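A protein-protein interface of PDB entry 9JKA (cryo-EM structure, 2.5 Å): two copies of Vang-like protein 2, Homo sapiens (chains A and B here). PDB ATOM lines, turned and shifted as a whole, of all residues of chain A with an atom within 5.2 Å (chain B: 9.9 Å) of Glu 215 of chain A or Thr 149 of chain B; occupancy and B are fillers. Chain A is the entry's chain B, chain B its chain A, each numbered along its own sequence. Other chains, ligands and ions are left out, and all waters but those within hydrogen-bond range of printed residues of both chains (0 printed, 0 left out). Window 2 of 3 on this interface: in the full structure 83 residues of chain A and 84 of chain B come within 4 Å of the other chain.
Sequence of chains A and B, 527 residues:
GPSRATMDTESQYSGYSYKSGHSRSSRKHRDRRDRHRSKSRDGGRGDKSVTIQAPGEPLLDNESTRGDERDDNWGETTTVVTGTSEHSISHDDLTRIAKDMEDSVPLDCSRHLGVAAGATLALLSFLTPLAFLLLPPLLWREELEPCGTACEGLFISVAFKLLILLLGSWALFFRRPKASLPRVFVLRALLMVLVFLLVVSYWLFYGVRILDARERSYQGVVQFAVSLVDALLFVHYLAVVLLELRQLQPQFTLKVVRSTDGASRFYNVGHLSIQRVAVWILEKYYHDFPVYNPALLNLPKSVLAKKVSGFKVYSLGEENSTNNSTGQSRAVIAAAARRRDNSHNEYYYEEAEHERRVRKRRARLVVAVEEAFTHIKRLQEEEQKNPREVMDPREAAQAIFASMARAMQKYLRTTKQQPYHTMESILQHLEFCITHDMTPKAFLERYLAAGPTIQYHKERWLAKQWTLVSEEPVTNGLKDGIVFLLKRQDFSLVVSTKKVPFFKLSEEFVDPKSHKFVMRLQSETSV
The side-chain hydroxyl of Thr 149 of chain B is in hydrogen-bond range of the side-chain carboxylate of Glu 215 of chain A (3.5 Å). OE1 of Glu 152 of chain B lies within salt-bridge range of NH2 of Arg 209 of chain A, 2.6 Å away.
The indole nitrogen (NE1) of Trp 140 of chain A is in hydrogen-bond range of the backbone carbonyl oxygen (O) of Glu 215 of chain A, 2.7 Å away. The backbone NH of Glu 215 of chain A sits at hydrogen-bond distance from the backbone carbonyl oxygen of Ile 210 of chain A (3.1 Å). The side-chain sulfur (SG) of Cys 147 of chain B forms a disulfide with the side-chain sulfur (SG) of Cys 151 of chain B, at 2.0 Å.
Among the printed residues, merely in contact across the chains: Phe 205 of chain A with Thr 149 of chain B (3.2 Å), Phe 205 of chain A with Glu 152 of chain B (3.3 Å), Phe 205 of chain A with Gly 153 of chain B (3.6 Å), Phe 205 of chain A with Ile 156 of chain B (3.6 Å), Arg 209 of chain A with Thr 149 of chain B (3.3 Å) and Ile 210 of chain A with Thr 149 of chain B (3.9 Å).
Of the printed residues of chain B, Phe 205 of chain A touches Thr 149, Glu 152, Gly 153 and Ile 156. Of the printed residues of chain B, Arg 209 of chain A touches Thr 149 and Glu 152. Ile 210 of chain A touches just one residue of chain B: Thr 149. No residue of chain B comes within 4 Å of Ala 213 of chain A. Glu 215 of chain A touches just one residue of chain B: Thr 149. Arg 216 of chain A touches none of the printed residues of chain B. Cys 147 of chain B touches none of the printed residues of chain A. Thr 149 of chain B touches just these residues of chain A: Phe 205, Arg 209, Ile 210 and Glu 215. Printed residues of chain A within 4 Å of Glu 152 of chain B: Phe 205 (3.3 Å) and Arg 209 (2.6 Å). Printed residues of chain A within 4 Å of Gly 153 of chain B: Phe 205 (3.6 Å). The nearest residue of chain B that does not touch Glu 215 of chain A is Gly 148 of chain B (5.4 Å). The nearest printed residue of chain A that does not touch Ile 156 of chain B is Arg 209 of chain A (7.7 Å).
Of the 15 printed residues of chain B, 4 touch a printed residue of chain A. Hydrophobic or aromatic side chains of chain B that line the printed part of chain A: Ile 156. Along chain A the printed residues that touch a printed residue of chain B span positions 205 to 215.
No position is printed for both chains.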
ATOM      1  N   TRP A 140     -19.962   9.547  25.425  1.00  0.00           N
ATOM      2  CA  TRP A 140     -20.697   9.568  26.691  1.00  0.00           C
ATOM      3  C   TRP A 140     -19.685   9.426  27.830  1.00  0.00           C
ATOM      4  O   TRP A 140     -19.387   8.334  28.313  1.00  0.00           O
ATOM      5  CB  TRP A 140     -21.824   8.496  26.719  1.00  0.00           C
ATOM      6  CG  TRP A 140     -21.446   7.038  26.506  1.00  0.00           C
ATOM      7  CD1 TRP A 140     -21.213   6.097  27.472  1.00  0.00           C
ATOM      8  CD2 TRP A 140     -21.276   6.368  25.254  1.00  0.00           C
ATOM      9  NE1 TRP A 140     -20.901   4.892  26.899  1.00  0.00           N
ATOM     10  CE2 TRP A 140     -20.934   5.029  25.537  1.00  0.00           C
ATOM     11  CE3 TRP A 140     -21.378   6.767  23.921  1.00  0.00           C
ATOM     12  CZ2 TRP A 140     -20.692   4.093  24.537  1.00  0.00           C
ATOM     13  CZ3 TRP A 140     -21.135   5.838  22.929  1.00  0.00           C
ATOM     14  CH2 TRP A 140     -20.798   4.516  23.241  1.00  0.00           C
ATOM     15  N   LEU A 144     -20.676   7.320  31.424  1.00  0.00           N
ATOM     16  CA  LEU A 144     -19.824   6.145  31.529  1.00  0.00           C
ATOM     17  C   LEU A 144     -19.541   5.796  32.986  1.00  0.00           C
ATOM     18  O   LEU A 144     -19.266   6.673  33.810  1.00  0.00           O
ATOM     19  CB  LEU A 144     -18.511   6.405  30.798  1.00  0.00           C
ATOM     20  CG  LEU A 144     -17.573   5.240  30.529  1.00  0.00           C
ATOM     21  CD1 LEU A 144     -18.246   4.297  29.553  1.00  0.00           C
ATOM     22  CD2 LEU A 144     -16.266   5.769  29.974  1.00  0.00           C
ATOM     23  N   PHE A 205     -20.659  -5.341  15.837  1.00  0.00           N
ATOM     24  CA  PHE A 205     -21.061  -5.588  17.217  1.00  0.00           C
ATOM     25  C   PHE A 205     -20.869  -4.350  18.083  1.00  0.00           C
ATOM     26  O   PHE A 205     -21.721  -4.044  18.927  1.00  0.00           O
ATOM     27  CB  PHE A 205     -20.279  -6.754  17.804  1.00  0.00           C
ATOM     28  CG  PHE A 205     -20.677  -7.083  19.206  1.00  0.00           C
ATOM     29  CD1 PHE A 205     -21.858  -7.754  19.454  1.00  0.00           C
ATOM     30  CD2 PHE A 205     -19.888  -6.699  20.278  1.00  0.00           C
ATOM     31  CE1 PHE A 205     -22.236  -8.048  20.741  1.00  0.00           C
ATOM     32  CE2 PHE A 205     -20.261  -6.990  21.567  1.00  0.00           C
ATOM     33  CZ  PHE A 205     -21.437  -7.662  21.797  1.00  0.00           C
ATOM     34  N   ARG A 209     -24.336  -2.906  19.638  1.00  0.00           N
ATOM     35  CA  ARG A 209     -24.481  -3.305  21.032  1.00  0.00           C
ATOM     36  C   ARG A 209     -23.697  -2.464  22.026  1.00  0.00           C
ATOM     37  O   ARG A 209     -23.913  -2.621  23.232  1.00  0.00           O
ATOM     38  CB  ARG A 209     -24.090  -4.780  21.221  1.00  0.00           C
ATOM     39  CG  ARG A 209     -25.005  -5.752  20.498  1.00  0.00           C
ATOM     40  CD  ARG A 209     -26.401  -5.730  21.094  1.00  0.00           C
ATOM     41  NE  ARG A 209     -27.324  -6.585  20.358  1.00  0.00           N
ATOM     42  CZ  ARG A 209     -27.535  -7.868  20.628  1.00  0.00           C
ATOM     43  NH1 ARG A 209     -28.395  -8.569  19.903  1.00  0.00           N
ATOM     44  NH2 ARG A 209     -26.883  -8.451  21.624  1.00  0.00           N
ATOM     45  N   ILE A 210     -22.804  -1.583  21.580  1.00  0.00           N
ATOM     46  CA  ILE A 210     -22.059  -0.698  22.465  1.00  0.00           C
ATOM     47  C   ILE A 210     -22.278   0.767  22.101  1.00  0.00           C
ATOM     48  O   ILE A 210     -22.614   1.588  22.960  1.00  0.00           O
ATOM     49  CB  ILE A 210     -20.553  -1.044  22.474  1.00  0.00           C
ATOM     50  CG1 ILE A 210     -20.331  -2.442  23.052  1.00  0.00           C
ATOM     51  CG2 ILE A 210     -19.767  -0.024  23.274  1.00  0.00           C
ATOM     52  CD1 ILE A 210     -18.926  -2.964  22.878  1.00  0.00           C
ATOM     53  N   ALA A 213     -26.284   1.391  21.776  1.00  0.00           N
ATOM     54  CA  ALA A 213     -26.895   1.118  23.069  1.00  0.00           C
ATOM     55  C   ALA A 213     -26.345   1.989  24.190  1.00  0.00           C
ATOM     56  O   ALA A 213     -26.957   2.019  25.264  1.00  0.00           O
ATOM     57  CB  ALA A 213     -26.713  -0.357  23.434  1.00  0.00           C
ATOM     58  N   ARG A 214     -25.229   2.690  23.951  1.00  0.00           N
ATOM     59  CA  ARG A 214     -24.530   3.538  24.923  1.00  0.00           C
ATOM     60  C   ARG A 214     -24.164   2.742  26.180  1.00  0.00           C
ATOM     61  O   ARG A 214     -24.705   2.944  27.270  1.00  0.00           O
ATOM     62  CB  ARG A 214     -25.342   4.796  25.258  1.00  0.00           C
ATOM     63  CG  ARG A 214     -25.465   5.756  24.090  1.00  0.00           C
ATOM     64  CD  ARG A 214     -26.207   7.022  24.476  1.00  0.00           C
ATOM     65  NE  ARG A 214     -26.408   7.896  23.325  1.00  0.00           N
ATOM     66  CZ  ARG A 214     -25.537   8.816  22.923  1.00  0.00           C
ATOM     67  NH1 ARG A 214     -24.398   8.986  23.581  1.00  0.00           N
ATOM     68  NH2 ARG A 214     -25.803   9.565  21.863  1.00  0.00           N
ATOM     69  N   GLU A 215     -23.252   1.793  25.964  1.00  0.00           N
ATOM     70  CA  GLU A 215     -22.826   0.864  27.005  1.00  0.00           C
ATOM     71  C   GLU A 215     -22.142   1.589  28.157  1.00  0.00           C
ATOM     72  O   GLU A 215     -21.246   2.412  27.949  1.00  0.00           O
ATOM     73  CB  GLU A 215     -21.880  -0.181  26.409  1.00  0.00           C
ATOM     74  CG  GLU A 215     -21.358  -1.215  27.399  1.00  0.00           C
ATOM     75  CD  GLU A 215     -22.434  -2.156  27.907  1.00  0.00           C
ATOM     76  OE1 GLU A 215     -23.425  -2.388  27.182  1.00  0.00           O
ATOM     77  OE2 GLU A 215     -22.287  -2.667  29.037  1.00  0.00           O
ATOM     78  N   ARG A 216     -22.578   1.278  29.375  1.00  0.00           N
ATOM     79  CA  ARG A 216     -22.045   1.908  30.574  1.00  0.00           C
ATOM     80  C   ARG A 216     -20.861   1.144  31.150  1.00  0.00           C
ATOM     81  O   ARG A 216     -19.929   1.761  31.677  1.00  0.00           O
ATOM     82  CB  ARG A 216     -23.145   2.035  31.629  1.00  0.00           C
ATOM     83  CG  ARG A 216     -24.262   2.988  31.248  1.00  0.00           C
ATOM     84  CD  ARG A 216     -25.336   3.026  32.319  1.00  0.00           C
ATOM     85  NE  ARG A 216     -24.827   3.558  33.580  1.00  0.00           N
ATOM     86  CZ  ARG A 216     -24.810   4.849  33.893  1.00  0.00           C
ATOM     87  NH1 ARG A 216     -25.278   5.748  33.038  1.00  0.00           N
ATOM     88  NH2 ARG A 216     -24.324   5.243  35.062  1.00  0.00           N
ATOM     89  N   SER A 217     -20.880  -0.184  31.064  1.00  0.00           N
ATOM     90  CA  SER A 217     -19.809  -1.015  31.609  1.00  0.00           C
ATOM     91  C   SER A 217     -18.579  -0.875  30.724  1.00  0.00           C
ATOM     92  O   SER A 217     -18.431  -1.576  29.722  1.00  0.00           O
ATOM     93  CB  SER A 217     -20.255  -2.468  31.706  1.00  0.00           C
ATOM     94  OG  SER A 217     -19.212  -3.289  32.203  1.00  0.00           O
ATOM     95  N   VAL A 221     -16.002  -2.962  27.521  1.00  0.00           N
ATOM     96  CA  VAL A 221     -15.519  -2.365  26.278  1.00  0.00           C
ATOM     97  C   VAL A 221     -14.004  -2.507  26.169  1.00  0.00           C
ATOM     98  O   VAL A 221     -13.464  -2.802  25.091  1.00  0.00           O
ATOM     99  CB  VAL A 221     -15.970  -0.894  26.201  1.00  0.00           C
ATOM    100  CG1 VAL A 221     -15.446  -0.218  24.943  1.00  0.00           C
ATOM    101  CG2 VAL A 221     -17.485  -0.807  26.262  1.00  0.00           C
ATOM    102  N   PRO B 146     -27.912 -13.347  33.669  1.00  0.00           N
ATOM    103  CA  PRO B 146     -27.698 -12.619  32.416  1.00  0.00           C
ATOM    104  C   PRO B 146     -26.490 -11.705  32.522  1.00  0.00           C
ATOM    105  O   PRO B 146     -26.228 -11.095  33.562  1.00  0.00           O
ATOM    106  CB  PRO B 146     -28.994 -11.819  32.246  1.00  0.00           C
ATOM    107  CG  PRO B 146     -29.492 -11.626  33.640  1.00  0.00           C
ATOM    108  CD  PRO B 146     -29.102 -12.869  34.395  1.00  0.00           C
ATOM    109  N   CYS B 147     -25.742 -11.622  31.426  1.00  0.00           N
ATOM    110  CA  CYS B 147     -24.554 -10.786  31.370  1.00  0.00           C
ATOM    111  C   CYS B 147     -24.608  -9.927  30.116  1.00  0.00           C
ATOM    112  O   CYS B 147     -25.322 -10.234  29.156  1.00  0.00           O
ATOM    113  CB  CYS B 147     -23.271 -11.626  31.409  1.00  0.00           C
ATOM    114  SG  CYS B 147     -23.068 -12.754  30.022  1.00  0.00           S
ATOM    115  N   GLY B 148     -23.838  -8.842  30.134  1.00  0.00           N
ATOM    116  CA  GLY B 148     -23.940  -7.823  29.110  1.00  0.00           C
ATOM    117  C   GLY B 148     -23.272  -8.141  27.789  1.00  0.00           C
ATOM    118  O   GLY B 148     -23.140  -9.307  27.403  1.00  0.00           O
ATOM    119  N   THR B 149     -22.840  -7.093  27.087  1.00  0.00           N
ATOM    120  CA  THR B 149     -22.251  -7.239  25.763  1.00  0.00           C
ATOM    121  C   THR B 149     -20.818  -7.749  25.803  1.00  0.00           C
ATOM    122  O   THR B 149     -20.284  -8.130  24.752  1.00  0.00           O
ATOM    123  CB  THR B 149     -22.292  -5.900  25.029  1.00  0.00           C
ATOM    124  OG1 THR B 149     -21.513  -4.939  25.751  1.00  0.00           O
ATOM    125  CG2 THR B 149     -23.721  -5.407  24.932  1.00  0.00           C
ATOM    126  N   ALA B 150     -20.187  -7.750  26.981  1.00  0.00           N
ATOM    127  CA  ALA B 150     -18.842  -8.298  27.110  1.00  0.00           C
ATOM    128  C   ALA B 150     -18.827  -9.790  26.806  1.00  0.00           C
ATOM    129  O   ALA B 150     -17.903 -10.285  26.147  1.00  0.00           O
ATOM    130  CB  ALA B 150     -18.298  -8.028  28.513  1.00  0.00           C
ATOM    131  N   CYS B 151     -19.874 -10.504  27.236  1.00  0.00           N
ATOM    132  CA  CYS B 151     -19.998 -11.930  26.950  1.00  0.00           C
ATOM    133  C   CYS B 151     -20.098 -12.190  25.453  1.00  0.00           C
ATOM    134  O   CYS B 151     -19.407 -13.064  24.922  1.00  0.00           O
ATOM    135  CB  CYS B 151     -21.219 -12.505  27.665  1.00  0.00           C
ATOM    136  SG  CYS B 151     -21.134 -12.496  29.461  1.00  0.00           S
ATOM    137  N   GLU B 152     -20.918 -11.407  24.749  1.00  0.00           N
ATOM    138  CA  GLU B 152     -21.110 -11.623  23.317  1.00  0.00           C
ATOM    139  C   GLU B 152     -19.879 -11.221  22.508  1.00  0.00           C
ATOM    140  O   GLU B 152     -19.555 -11.876  21.504  1.00  0.00           O
ATOM    141  CB  GLU B 152     -22.345 -10.860  22.849  1.00  0.00           C
ATOM    142  CG  GLU B 152     -23.640 -11.366  23.455  1.00  0.00           C
ATOM    143  CD  GLU B 152     -24.840 -10.537  23.046  1.00  0.00           C
ATOM    144  OE1 GLU B 152     -24.649  -9.479  22.410  1.00  0.00           O
ATOM    145  OE2 GLU B 152     -25.977 -10.945  23.361  1.00  0.00           O
ATOM    146  N   GLY B 153     -19.172 -10.170  22.936  1.00  0.00           N
ATOM    147  CA  GLY B 153     -17.894  -9.851  22.315  1.00  0.00           C
ATOM    148  C   GLY B 153     -16.866 -10.948  22.516  1.00  0.00           C
ATOM    149  O   GLY B 153     -16.084 -11.263  21.610  1.00  0.00           O
ATOM    150  N   LEU B 154     -16.883 -11.582  23.689  1.00  0.00           N
ATOM    151  CA  LEU B 154     -15.998 -12.720  23.891  1.00  0.00           C
ATOM    152  C   LEU B 154     -16.454 -13.949  23.107  1.00  0.00           C
ATOM    153  O   LEU B 154     -15.616 -14.780  22.750  1.00  0.00           O
ATOM    154  CB  LEU B 154     -15.870 -13.028  25.377  1.00  0.00           C
ATOM    155  CG  LEU B 154     -15.116 -11.980  26.195  1.00  0.00           C
ATOM    156  CD1 LEU B 154     -15.218 -12.303  27.665  1.00  0.00           C
ATOM    157  CD2 LEU B 154     -13.664 -11.873  25.764  1.00  0.00           C
ATOM    158  N   PHE B 155     -17.754 -14.076  22.811  1.00  0.00           N
ATOM    159  CA  PHE B 155     -18.204 -15.126  21.890  1.00  0.00           C
ATOM    160  C   PHE B 155     -17.640 -14.907  20.492  1.00  0.00           C
ATOM    161  O   PHE B 155     -17.242 -15.862  19.810  1.00  0.00           O
ATOM    162  CB  PHE B 155     -19.732 -15.198  21.801  1.00  0.00           C
ATOM    163  CG  PHE B 155     -20.399 -15.889  22.954  1.00  0.00           C
ATOM    164  CD1 PHE B 155     -20.236 -17.249  23.149  1.00  0.00           C
ATOM    165  CD2 PHE B 155     -21.292 -15.209  23.762  1.00  0.00           C
ATOM    166  CE1 PHE B 155     -20.876 -17.894  24.190  1.00  0.00           C
ATOM    167  CE2 PHE B 155     -21.932 -15.840  24.804  1.00  0.00           C
ATOM    168  CZ  PHE B 155     -21.728 -17.187  25.015  1.00  0.00           C
ATOM    169  N   ILE B 156     -17.616 -13.648  20.047  1.00  0.00           N
ATOM    170  CA  ILE B 156     -17.023 -13.312  18.751  1.00  0.00           C
ATOM    171  C   ILE B 156     -15.531 -13.629  18.744  1.00  0.00           C
ATOM    172  O   ILE B 156     -14.994 -14.170  17.762  1.00  0.00           O
ATOM    173  CB  ILE B 156     -17.296 -11.834  18.416  1.00  0.00           C
ATOM    174  CG1 ILE B 156     -18.796 -11.608  18.279  1.00  0.00           C
ATOM    175  CG2 ILE B 156     -16.595 -11.411  17.137  1.00  0.00           C
ATOM    176  CD1 ILE B 156     -19.173 -10.171  18.230  1.00  0.00           C
ATOM    177  N   SER B 157     -14.848 -13.329  19.856  1.00  0.00           N
ATOM    178  CA  SER B 157     -13.424 -13.639  19.955  1.00  0.00           C
ATOM    179  C   SER B 157     -13.177 -15.144  19.944  1.00  0.00           C
ATOM    180  O   SER B 157     -12.234 -15.609  19.297  1.00  0.00           O
ATOM    181  CB  SER B 157     -12.827 -13.020  21.216  1.00  0.00           C
ATOM    182  OG  SER B 157     -13.256 -13.718  22.369  1.00  0.00           O
ATOM    183  N   GLN B 219     -20.211 -14.817  32.731  1.00  0.00           N
ATOM    184  CA  GLN B 219     -19.071 -14.059  32.223  1.00  0.00           C
ATOM    185  C   GLN B 219     -17.757 -14.749  32.563  1.00  0.00           C
ATOM    186  O   GLN B 219     -16.838 -14.782  31.735  1.00  0.00           O
ATOM    187  CB  GLN B 219     -19.093 -12.641  32.792  1.00  0.00           C
ATOM    188  CG  GLN B 219     -17.985 -11.739  32.276  1.00  0.00           C
ATOM    189  CD  GLN B 219     -18.053 -10.341  32.858  1.00  0.00           C
ATOM    190  OE1 GLN B 219     -18.915 -10.040  33.681  1.00  0.00           O
ATOM    191  NE2 GLN B 219     -17.135  -9.479  32.435  1.00  0.00           N
ATOM    192  N   VAL B 222     -17.383 -17.709  30.151  1.00  0.00           N
ATOM    193  CA  VAL B 222     -16.991 -17.327  28.799  1.00  0.00           C
ATOM    194  C   VAL B 222     -15.541 -16.842  28.775  1.00  0.00           C
ATOM    195  O   VAL B 222     -14.796 -17.146  27.837  1.00  0.00           O
ATOM    196  CB  VAL B 222     -17.975 -16.287  28.231  1.00  0.00           C
ATOM    197  CG1 VAL B 222     -17.593 -15.887  26.832  1.00  0.00           C
ATOM    198  CG2 VAL B 222     -19.359 -16.866  28.195  1.00  0.00           C
ATOM    199  N   GLN B 223     -15.099 -16.127  29.821  1.00  0.00           N
ATOM    200  CA  GLN B 223     -13.681 -15.782  29.946  1.00  0.00           C
ATOM    201  C   GLN B 223     -12.805 -17.017  30.112  1.00  0.00           C
ATOM    202  O   GLN B 223     -11.667 -17.042  29.629  1.00  0.00           O
ATOM    203  CB  GLN B 223     -13.454 -14.846  31.131  1.00  0.00           C
ATOM    204  CG  GLN B 223     -13.961 -13.437  30.940  1.00  0.00           C
ATOM    205  CD  GLN B 223     -13.730 -12.573  32.159  1.00  0.00           C
ATOM    206  OE1 GLN B 223     -13.251 -13.050  33.188  1.00  0.00           O
ATOM    207  NE2 GLN B 223     -14.070 -11.295  32.053  1.00  0.00           N
